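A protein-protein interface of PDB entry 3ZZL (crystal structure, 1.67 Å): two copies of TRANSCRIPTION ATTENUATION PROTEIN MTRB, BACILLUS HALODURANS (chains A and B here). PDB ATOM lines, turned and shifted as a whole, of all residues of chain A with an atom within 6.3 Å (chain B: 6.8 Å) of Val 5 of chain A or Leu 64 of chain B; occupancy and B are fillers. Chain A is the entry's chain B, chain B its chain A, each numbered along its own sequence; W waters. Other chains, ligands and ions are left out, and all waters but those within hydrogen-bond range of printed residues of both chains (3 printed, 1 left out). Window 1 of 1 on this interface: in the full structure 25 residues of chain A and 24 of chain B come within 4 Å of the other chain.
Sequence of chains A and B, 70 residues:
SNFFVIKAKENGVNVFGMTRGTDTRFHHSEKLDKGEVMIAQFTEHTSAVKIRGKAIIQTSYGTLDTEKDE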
ATOM      1  N   PHE A   3       7.437 -16.625 -29.426  1.00  0.00           N
ATOM      2  CA  PHE A   3       7.549 -18.085 -29.592  1.00  0.00           C
ATOM      3  C   PHE A   3       6.175 -18.734 -29.528  1.00  0.00           C
ATOM      4  O   PHE A   3       5.223 -18.155 -28.998  1.00  0.00           O
ATOM      5  CB  PHE A   3       8.428 -18.745 -28.518  1.00  0.00           C
ATOM      6  CG  PHE A   3       7.778 -18.844 -27.151  1.00  0.00           C
ATOM      7  CD1 PHE A   3       7.658 -17.718 -26.323  1.00  0.00           C
ATOM      8  CD2 PHE A   3       7.293 -20.054 -26.690  1.00  0.00           C
ATOM      9  CE1 PHE A   3       7.050 -17.819 -25.065  1.00  0.00           C
ATOM     10  CE2 PHE A   3       6.681 -20.157 -25.451  1.00  0.00           C
ATOM     11  CZ  PHE A   3       6.568 -19.045 -24.633  1.00  0.00           C
ATOM     12  N   PHE A   4       6.117 -19.965 -30.032  1.00  0.00           N
ATOM     13  CA  PHE A   4       4.896 -20.753 -30.103  1.00  0.00           C
ATOM     14  C   PHE A   4       5.212 -22.196 -29.714  1.00  0.00           C
ATOM     15  O   PHE A   4       6.368 -22.638 -29.845  1.00  0.00           O
ATOM     16  CB  PHE A   4       4.320 -20.683 -31.530  1.00  0.00           C
ATOM     17  CG  PHE A   4       5.376 -20.572 -32.607  1.00  0.00           C
ATOM     18  CD1 PHE A   4       5.955 -19.353 -32.914  1.00  0.00           C
ATOM     19  CD2 PHE A   4       5.782 -21.688 -33.307  1.00  0.00           C
ATOM     20  CE1 PHE A   4       6.937 -19.267 -33.891  1.00  0.00           C
ATOM     21  CE2 PHE A   4       6.743 -21.609 -34.274  1.00  0.00           C
ATOM     22  CZ  PHE A   4       7.324 -20.395 -34.570  1.00  0.00           C
ATOM     23  N   VAL A   5       4.200 -22.914 -29.248  1.00  0.00           N
ATOM     24  CA  VAL A   5       4.319 -24.310 -28.865  1.00  0.00           C
ATOM     25  C   VAL A   5       3.348 -25.155 -29.696  1.00  0.00           C
ATOM     26  O   VAL A   5       2.169 -24.798 -29.842  1.00  0.00           O
ATOM     27  CB  VAL A   5       3.982 -24.481 -27.368  1.00  0.00           C
ATOM     28  CG1 VAL A   5       4.170 -25.929 -26.907  1.00  0.00           C
ATOM     29  CG2 VAL A   5       4.829 -23.513 -26.515  1.00  0.00           C
ATOM     30  N   ILE A   6       3.822 -26.291 -30.187  1.00  0.00           N
ATOM     31  CA  ILE A   6       2.981 -27.254 -30.894  1.00  0.00           C
ATOM     32  C   ILE A   6       3.130 -28.631 -30.257  1.00  0.00           C
ATOM     33  O   ILE A   6       4.239 -29.129 -30.149  1.00  0.00           O
ATOM     34  CB  ILE A   6       3.381 -27.404 -32.373  1.00  0.00           C
ATOM     35  CG1 ILE A   6       3.431 -26.043 -33.086  1.00  0.00           C
ATOM     36  CG2 ILE A   6       2.427 -28.356 -33.080  1.00  0.00           C
ATOM     37  CD1 ILE A   6       4.797 -25.603 -33.375  1.00  0.00           C
ATOM     38  N   LYS A   7       2.030 -29.223 -29.807  1.00  0.00           N
ATOM     39  CA  LYS A   7       2.029 -30.614 -29.343  1.00  0.00           C
ATOM     40  C   LYS A   7       1.223 -31.476 -30.309  1.00  0.00           C
ATOM     41  O   LYS A   7       0.066 -31.171 -30.574  1.00  0.00           O
ATOM     42  CB  LYS A   7       1.412 -30.709 -27.941  1.00  0.00           C
ATOM     43  CG  LYS A   7       1.272 -32.135 -27.388  1.00  0.00           C
ATOM     44  CD  LYS A   7       0.622 -32.151 -26.006  1.00  0.00           C
ATOM     45  CE  LYS A   7      -0.071 -33.474 -25.745  1.00  0.00           C
ATOM     46  NZ  LYS A   7      -0.725 -33.529 -24.399  1.00  0.00           N
ATOM     47  N   VAL A  37       6.588 -32.495 -28.877  1.00  0.00           N
ATOM     48  CA  VAL A  37       6.344 -31.078 -28.720  1.00  0.00           C
ATOM     49  C   VAL A  37       7.475 -30.312 -29.380  1.00  0.00           C
ATOM     50  O   VAL A  37       8.644 -30.670 -29.243  1.00  0.00           O
ATOM     51  CB  VAL A  37       6.225 -30.653 -27.228  1.00  0.00           C
ATOM     52  CG1 VAL A  37       6.175 -29.127 -27.102  1.00  0.00           C
ATOM     53  CG2 VAL A  37       4.997 -31.310 -26.565  1.00  0.00           C
ATOM     54  N   MET A  38       7.114 -29.273 -30.118  1.00  0.00           N
ATOM     55  CA  MET A  38       8.086 -28.323 -30.626  1.00  0.00           C
ATOM     56  C   MET A  38       7.801 -26.962 -30.006  1.00  0.00           C
ATOM     57  O   MET A  38       6.664 -26.497 -30.004  1.00  0.00           O
ATOM     58  CB  MET A  38       8.006 -28.234 -32.141  1.00  0.00           C
ATOM     59  CG  MET A  38       9.018 -27.279 -32.818  1.00  0.00           C
ATOM     60  SD  MET A  38       8.875 -27.448 -34.632  1.00  0.00           S
ATOM     61  CE  MET A  38      10.050 -26.258 -35.234  1.00  0.00           C
ATOM     62  N   ILE A  39       8.859 -26.306 -29.531  1.00  0.00           N
ATOM     63  CA  ILE A  39       8.777 -24.937 -29.054  1.00  0.00           C
ATOM     64  C   ILE A  39       9.708 -24.169 -29.961  1.00  0.00           C
ATOM     65  O   ILE A  39      10.871 -24.522 -30.093  1.00  0.00           O
ATOM     66  CB  ILE A  39       9.233 -24.782 -27.579  1.00  0.00           C
ATOM     67  CG1 ILE A  39       8.495 -25.765 -26.656  1.00  0.00           C
ATOM     68  CG2 ILE A  39       8.968 -23.360 -27.103  1.00  0.00           C
ATOM     69  CD1 ILE A  39       9.096 -25.798 -25.266  1.00  0.00           C
ATOM     70  N   ALA A  40       9.209 -23.136 -30.622  1.00  0.00           N
ATOM     71  CA  ALA A  40      10.042 -22.481 -31.638  1.00  0.00           C
ATOM     72  C   ALA A  40       9.776 -20.984 -31.663  1.00  0.00           C
ATOM     73  O   ALA A  40       8.709 -20.524 -31.293  1.00  0.00           O
ATOM     74  CB  ALA A  40       9.787 -23.100 -33.042  1.00  0.00           C
ATOM     75  N   ILE A  56      -2.225 -29.546 -30.707  1.00  0.00           N
ATOM     76  CA  ILE A  56      -2.484 -28.468 -29.760  1.00  0.00           C
ATOM     77  C   ILE A  56      -1.453 -27.393 -30.042  1.00  0.00           C
ATOM     78  O   ILE A  56      -0.271 -27.688 -30.152  1.00  0.00           O
ATOM     79  CB  ILE A  56      -2.330 -28.946 -28.308  1.00  0.00           C
ATOM     80  CG1 ILE A  56      -3.511 -29.836 -27.916  1.00  0.00           C
ATOM     81  CG2 ILE A  56      -2.209 -27.765 -27.356  1.00  0.00           C
ATOM     82  CD1 ILE A  56      -4.878 -29.215 -28.207  1.00  0.00           C
ATOM     83  N   ILE A  57      -1.911 -26.154 -30.193  1.00  0.00           N
ATOM     84  CA  ILE A  57      -1.032 -25.042 -30.563  1.00  0.00           C
ATOM     85  C   ILE A  57      -1.167 -23.973 -29.490  1.00  0.00           C
ATOM     86  O   ILE A  57      -2.282 -23.652 -29.101  1.00  0.00           O
ATOM     87  CB  ILE A  57      -1.417 -24.458 -31.931  1.00  0.00           C
ATOM     88  CG1 ILE A  57      -1.186 -25.511 -33.028  1.00  0.00           C
ATOM     89  CG2 ILE A  57      -0.583 -23.188 -32.220  1.00  0.00           C
ATOM     90  CD1 ILE A  57      -1.853 -25.180 -34.358  1.00  0.00           C
ATOM     91  N   GLN A  58      -0.045 -23.457 -28.999  1.00  0.00           N
ATOM     92  CA  GLN A  58      -0.048 -22.387 -27.985  1.00  0.00           C
ATOM     93  C   GLN A  58       0.732 -21.170 -28.426  1.00  0.00           C
ATOM     94  O   GLN A  58       1.865 -21.281 -28.917  1.00  0.00           O
ATOM     95  CB  GLN A  58       0.540 -22.870 -26.664  1.00  0.00           C
ATOM     96  CG  GLN A  58      -0.311 -23.829 -25.929  1.00  0.00           C
ATOM     97  CD  GLN A  58       0.287 -24.207 -24.583  1.00  0.00           C
ATOM     98  OE1 GLN A  58       1.507 -24.175 -24.396  1.00  0.00           O
ATOM     99  NE2 GLN A  58      -0.576 -24.590 -23.645  1.00  0.00           N
ATOM    100  N   THR A  59       0.091 -20.008 -28.285  1.00  0.00           N
ATOM    101  CA  THR A  59       0.719 -18.714 -28.476  1.00  0.00           C
ATOM    102  C   THR A  59       0.309 -17.826 -27.307  1.00  0.00           C
ATOM    103  O   THR A  59      -0.487 -18.237 -26.460  1.00  0.00           O
ATOM    104  CB  THR A  59       0.279 -18.035 -29.788  1.00  0.00           C
ATOM    105  OG1 THR A  59      -1.040 -17.508 -29.628  1.00  0.00           O
ATOM    106  CG2 THR A  59       0.319 -19.023 -30.963  1.00  0.00           C
ATOM    107  N   ALA B  55       6.729 -36.283 -20.624  1.00  0.00           N
ATOM    108  CA  ALA B  55       7.299 -35.100 -19.980  1.00  0.00           C
ATOM    109  C   ALA B  55       6.251 -34.056 -19.610  1.00  0.00           C
ATOM    110  O   ALA B  55       5.175 -33.983 -20.222  1.00  0.00           O
ATOM    111  CB  ALA B  55       8.375 -34.465 -20.892  1.00  0.00           C
ATOM    112  N   ILE B  56       6.575 -33.283 -18.583  1.00  0.00           N
ATOM    113  CA  ILE B  56       5.875 -32.059 -18.217  1.00  0.00           C
ATOM    114  C   ILE B  56       6.709 -30.898 -18.777  1.00  0.00           C
ATOM    115  O   ILE B  56       7.921 -30.857 -18.592  1.00  0.00           O
ATOM    116  CB  ILE B  56       5.766 -31.923 -16.682  1.00  0.00           C
ATOM    117  CG1 ILE B  56       4.874 -33.030 -16.104  1.00  0.00           C
ATOM    118  CG2 ILE B  56       5.247 -30.549 -16.295  1.00  0.00           C
ATOM    119  CD1 ILE B  56       3.510 -33.127 -16.753  1.00  0.00           C
ATOM    120  N   ILE B  57       6.067 -29.972 -19.488  1.00  0.00           N
ATOM    121  CA  ILE B  57       6.771 -28.860 -20.139  1.00  0.00           C
ATOM    122  C   ILE B  57       6.149 -27.556 -19.669  1.00  0.00           C
ATOM    123  O   ILE B  57       4.941 -27.435 -19.632  1.00  0.00           O
ATOM    124  CB  ILE B  57       6.670 -28.967 -21.666  1.00  0.00           C
ATOM    125  CG1 ILE B  57       7.341 -30.273 -22.129  1.00  0.00           C
ATOM    126  CG2 ILE B  57       7.292 -27.722 -22.344  1.00  0.00           C
ATOM    127  CD1 ILE B  57       6.888 -30.785 -23.469  1.00  0.00           C
ATOM    128  N   GLN B  58       6.979 -26.594 -19.295  1.00  0.00           N
ATOM    129  CA  GLN B  58       6.501 -25.288 -18.836  1.00  0.00           C
ATOM    130  C   GLN B  58       7.090 -24.191 -19.684  1.00  0.00           C
ATOM    131  O   GLN B  58       8.292 -24.168 -19.920  1.00  0.00           O
ATOM    132  CB  GLN B  58       6.936 -25.027 -17.393  1.00  0.00           C
ATOM    133  CG  GLN B  58       6.146 -25.692 -16.338  1.00  0.00           C
ATOM    134  CD  GLN B  58       6.541 -25.201 -14.952  1.00  0.00           C
ATOM    135  OE1 GLN B  58       7.695 -24.847 -14.709  1.00  0.00           O
ATOM    136  NE2 GLN B  58       5.580 -25.165 -14.046  1.00  0.00           N
ATOM    137  N   THR B  59       6.239 -23.278 -20.141  1.00  0.00           N
ATOM    138  CA  THR B  59       6.680 -22.061 -20.797  1.00  0.00           C
ATOM    139  C   THR B  59       5.859 -20.927 -20.209  1.00  0.00           C
ATOM    140  O   THR B  59       5.049 -21.152 -19.318  1.00  0.00           O
ATOM    141  CB  THR B  59       6.407 -22.106 -22.317  1.00  0.00           C
ATOM    142  OG1 THR B  59       5.003 -22.006 -22.542  1.00  0.00           O
ATOM    143  CG2 THR B  59       6.933 -23.396 -22.938  1.00  0.00           C
ATOM    144  N   TYR B  61       3.287 -19.771 -21.418  1.00  0.00           N
ATOM    145  CA  TYR B  61       1.887 -20.041 -21.735  1.00  0.00           C
ATOM    146  C   TYR B  61       1.245 -21.087 -20.850  1.00  0.00           C
ATOM    147  O   TYR B  61       0.038 -21.296 -20.925  1.00  0.00           O
ATOM    148  CB  TYR B  61       1.747 -20.464 -23.197  1.00  0.00           C
ATOM    149  CG  TYR B  61       2.433 -19.521 -24.170  1.00  0.00           C
ATOM    150  CD1 TYR B  61       2.503 -18.145 -23.920  1.00  0.00           C
ATOM    151  CD2 TYR B  61       2.966 -19.995 -25.359  1.00  0.00           C
ATOM    152  CE1 TYR B  61       3.133 -17.280 -24.829  1.00  0.00           C
ATOM    153  CE2 TYR B  61       3.590 -19.143 -26.256  1.00  0.00           C
ATOM    154  CZ  TYR B  61       3.661 -17.790 -25.987  1.00  0.00           C
ATOM    155  OH  TYR B  61       4.280 -16.948 -26.880  1.00  0.00           O
ATOM    156  N   GLY B  62       2.043 -21.734 -20.006  1.00  0.00           N
ATOM    157  CA  GLY B  62       1.503 -22.661 -19.020  1.00  0.00           C
ATOM    158  C   GLY B  62       2.232 -23.984 -19.046  1.00  0.00           C
ATOM    159  O   GLY B  62       3.302 -24.106 -19.652  1.00  0.00           O
ATOM    160  N   THR B  63       1.625 -24.968 -18.392  1.00  0.00           N
ATOM    161  CA  THR B  63       2.198 -26.291 -18.243  1.00  0.00           C
ATOM    162  C   THR B  63       1.498 -27.273 -19.173  1.00  0.00           C
ATOM    163  O   THR B  63       0.269 -27.309 -19.253  1.00  0.00           O
ATOM    164  CB  THR B  63       2.091 -26.767 -16.782  1.00  0.00           C
ATOM    165  OG1 THR B  63       2.843 -25.875 -15.949  1.00  0.00           O
ATOM    166  CG2 THR B  63       2.616 -28.196 -16.624  1.00  0.00           C
ATOM    167  N   LEU B  64       2.307 -28.073 -19.856  1.00  0.00           N
ATOM    168  CA  LEU B  64       1.855 -29.016 -20.858  1.00  0.00           C
ATOM    169  C   LEU B  64       2.335 -30.399 -20.433  1.00  0.00           C
ATOM    170  O   LEU B  64       3.471 -30.546 -19.987  1.00  0.00           O
ATOM    171  CB  LEU B  64       2.462 -28.628 -22.212  1.00  0.00           C
ATOM    172  CG  LEU B  64       1.655 -28.842 -23.482  1.00  0.00           C
ATOM    173  CD1 LEU B  64       0.226 -28.312 -23.350  1.00  0.00           C
ATOM    174  CD2 LEU B  64       2.384 -28.187 -24.660  1.00  0.00           C
ATOM    175  N   ASP B  65       1.453 -31.392 -20.524  1.00  0.00           N
ATOM    176  CA  ASP B  65       1.788 -32.785 -20.244  1.00  0.00           C
ATOM    177  C   ASP B  65       1.736 -33.562 -21.551  1.00  0.00           C
ATOM    178  O   ASP B  65       0.684 -33.613 -22.194  1.00  0.00           O
ATOM    179  CB  ASP B  65       0.776 -33.351 -19.238  1.00  0.00           C
ATOM    180  CG  ASP B  65       1.060 -34.796 -18.836  1.00  0.00           C
ATOM    181  OD1 ASP B  65       1.836 -35.499 -19.522  1.00  0.00           O
ATOM    182  OD2 ASP B  65       0.465 -35.239 -17.828  1.00  0.00           O
ATOM    183  N   THR B  66       2.851 -34.178 -21.943  1.00  0.00           N
ATOM    184  CA  THR B  66       2.930 -34.840 -23.248  1.00  0.00           C
ATOM    185  C   THR B  66       2.007 -36.064 -23.353  1.00  0.00           C
ATOM    186  O   THR B  66       1.582 -36.407 -24.451  1.00  0.00           O
ATOM    187  CB  THR B  66       4.348 -35.301 -23.591  1.00  0.00           C
ATOM    188  OG1 THR B  66       4.782 -36.269 -22.632  1.00  0.00           O
ATOM    189  CG2 THR B  66       5.321 -34.117 -23.629  1.00  0.00           C
ATOM    190  N   GLU B  67       1.726 -36.721 -22.223  1.00  0.00           N
ATOM    191  CA  GLU B  67       0.876 -37.926 -22.190  1.00  0.00           C
ATOM    192  C   GLU B  67      -0.625 -37.641 -22.163  1.00  0.00           C
ATOM    193  O   GLU B  67      -1.435 -38.546 -22.411  1.00  0.00           O
ATOM    194  CB  GLU B  67       1.195 -38.778 -20.957  1.00  0.00           C
ATOM    195  CG  GLU B  67       2.554 -39.444 -20.958  1.00  0.00           C
ATOM    196  CD  GLU B  67       2.642 -40.546 -19.910  1.00  0.00           C
ATOM    197  OE1 GLU B  67       2.090 -41.642 -20.153  1.00  0.00           O
ATOM    198  OE2 GLU B  67       3.260 -40.319 -18.846  1.00  0.00           O
ATOM    199  N   LYS B  68      -0.999 -36.410 -21.824  1.00  0.00           N
ATOM    200  CA  LYS B  68      -2.406 -36.036 -21.691  1.00  0.00           C
ATOM    201  C   LYS B  68      -3.117 -36.065 -23.050  1.00  0.00           C
ATOM    202  O   LYS B  68      -2.505 -35.794 -24.093  1.00  0.00           O
ATOM    203  CB  LYS B  68      -2.523 -34.638 -21.069  1.00  0.00           C
ATOM    204  CG  LYS B  68      -3.939 -34.239 -20.637  1.00  0.00           C
ATOM    205  CD  LYS B  68      -4.161 -32.733 -20.750  1.00  0.00           C
ATOM    206  CE  LYS B  68      -5.646 -32.382 -20.711  1.00  0.00           C
ATOM    207  NZ  LYS B  68      -5.901 -30.985 -21.176  1.00  0.00           N
ATOM    208  N   GLU B  70      -5.723 -34.045 -24.970  1.00  0.00           N
ATOM    209  CA  GLU B  70      -6.529 -32.830 -25.148  1.00  0.00           C
ATOM    210  C   GLU B  70      -7.503 -33.006 -26.316  1.00  0.00           C
ATOM    211  O   GLU B  70      -8.087 -34.075 -26.507  1.00  0.00           O
ATOM    212  CB  GLU B  70      -5.646 -31.596 -25.387  1.00  0.00           C
ATOM    213  CG  GLU B  70      -4.748 -31.226 -24.217  1.00  0.00           C
ATOM    214  CD  GLU B  70      -3.319 -31.691 -24.390  1.00  0.00           C
ATOM    215  OE1 GLU B  70      -3.092 -32.671 -25.133  1.00  0.00           O
ATOM    216  OE2 GLU B  70      -2.420 -31.074 -23.778  1.00  0.00           O
ATOM    217  OXT GLU B  70      -7.732 -32.085 -27.103  1.00  0.00           O
HETATM  218  O   HOH W   1       3.040 -16.140 -29.136  1.00  0.00           O
HETATM  219  O   HOH W   2       3.625 -24.240 -22.598  1.00  0.00           O
HETATM  220  O   HOH W   3      -0.875 -25.314 -20.800  1.00  0.00           O
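O of Phe 3 of chain A lies within hydrogen-bond range of OH of Tyr 61 of chain B. OE1 of Glu 70 of chain B is in salt-bridge range of NZ of Lys 7 of chain A (2.6 Å). O of Asp 65 of chain B is in hydrogen-bond range of NZ of Lys 7 of chain A (2.6 Å). The backbone carbonyl oxygen (O) of Lys 68 of chain B is in hydrogen-bond range of the side-chain amino group (NZ) of Lys 7 of chain A (2.9 Å).
The side-chain carboxylate (OD1) of Asp 65 of chain B lies within hydrogen-bond range of the backbone NH (N) of Glu 67 of chain B (3.0 Å). O of Leu 64 of chain B is in hydrogen-bond range of N of Ile 57 of chain B, 2.7 Å away. OG1 of Thr 59 of chain B sits at hydrogen-bond distance from N of Tyr 61 of chain B, at 3.0 Å. The backbone carbonyl oxygen of Val 5 of chain A sits at hydrogen-bond distance from the backbone NH of Gln 58 of chain A, at 2.7 Å. O of Ile 56 of chain A lies within hydrogen-bond range of N of Lys 7 of chain A. The backbone NH (N) of Ala 55 of chain B sits at hydrogen-bond distance from the side-chain hydroxyl (OG1) of Thr 66 of chain B.
Among the printed residues, pairs that only touch across the chains: Phe 3 of chain A with Thr 59 of chain B, Val 5 of chain A with Leu 64 of chain B, Lys 7 of chain A with Thr 66 of chain B, Val 37 of chain A with Ile 57 of chain B, Ile 39 of chain A with Ile 57 of chain B, Ile 39 of chain A with Thr 59 of chain B, Ile 56 of chain A with Glu 70 of chain B, Gln 58 of chain A with Tyr 61 of chain B, Gln 58 of chain A with Leu 64 of chain B and Thr 59 of chain A with Tyr 61 of chain B.
Val 5 of chain A touches just one residue of chain B: Leu 64 (3.7 Å). Leu 64 of chain B touches just these residues of chain A: Val 5 and Gln 58. Of the printed residues of chain A, Ile 57 of chain B touches Val 37 and Ile 39. Printed residues of chain A within 4 Å of Glu 70 of chain B: Lys 7 (2.6 Å) and Ile 56 (3.7 Å). Printed residues of chain A within 4 Å of Lys 68 of chain B: Lys 7. Of the printed residues of chain B, Lys 7 of chain A touches Asp 65, Thr 66, Lys 68 and Glu 70. Of the printed residues of chain A, Asp 65 of chain B touches Lys 7 (2.6 Å). Thr 63 of chain B touches none of the printed residues of chain A. The nearest printed residue of chain B that does not touch Phe 3 of chain A is Gly 62 of chain B (7.0 Å).
Of the 13 printed residues of chain A, 8 touch a printed residue of chain B. Hydrophobic or aromatic side chains of chain A that line the printed part of chain B: Phe 3, Val 5, Val 37, Ile 39 and Ile 56. Of the 14 printed residues of chain B, 8 touch a printed residue of chain A. Among the printed residues, 14 pairs touch across the chains. Among the printed residues, Asp or Glu carboxylates within 4 Å of a Lys or Arg side-chain nitrogen of the other chain: Lys 7 of chain A with Glu 70 of chain B (2.6 Å).
Positions printed for both chains: 56, 57, 58 and 59. Of the 14 pairs that touch across the chains among the printed residues, none has its exchanged pair printed and touching as well.
Water W2 lies within hydrogen-bond range of the side-chain hydroxyl of Thr 59 of chain B (2.6 Å), the side-chain amide oxygen of Gln 58 of chain A (2.8 Å) and the backbone carbonyl oxygen of Gly 62 of chain B (3.0 Å). Water W1 lies within hydrogen-bond range of OH of Tyr 61 of chain B and O of Phe 3 of chain A. Water W3 bridges O of Thr 63 of chain B (2.8 Å) and NE2 of Gln 58 of chain A (3.0 Å).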
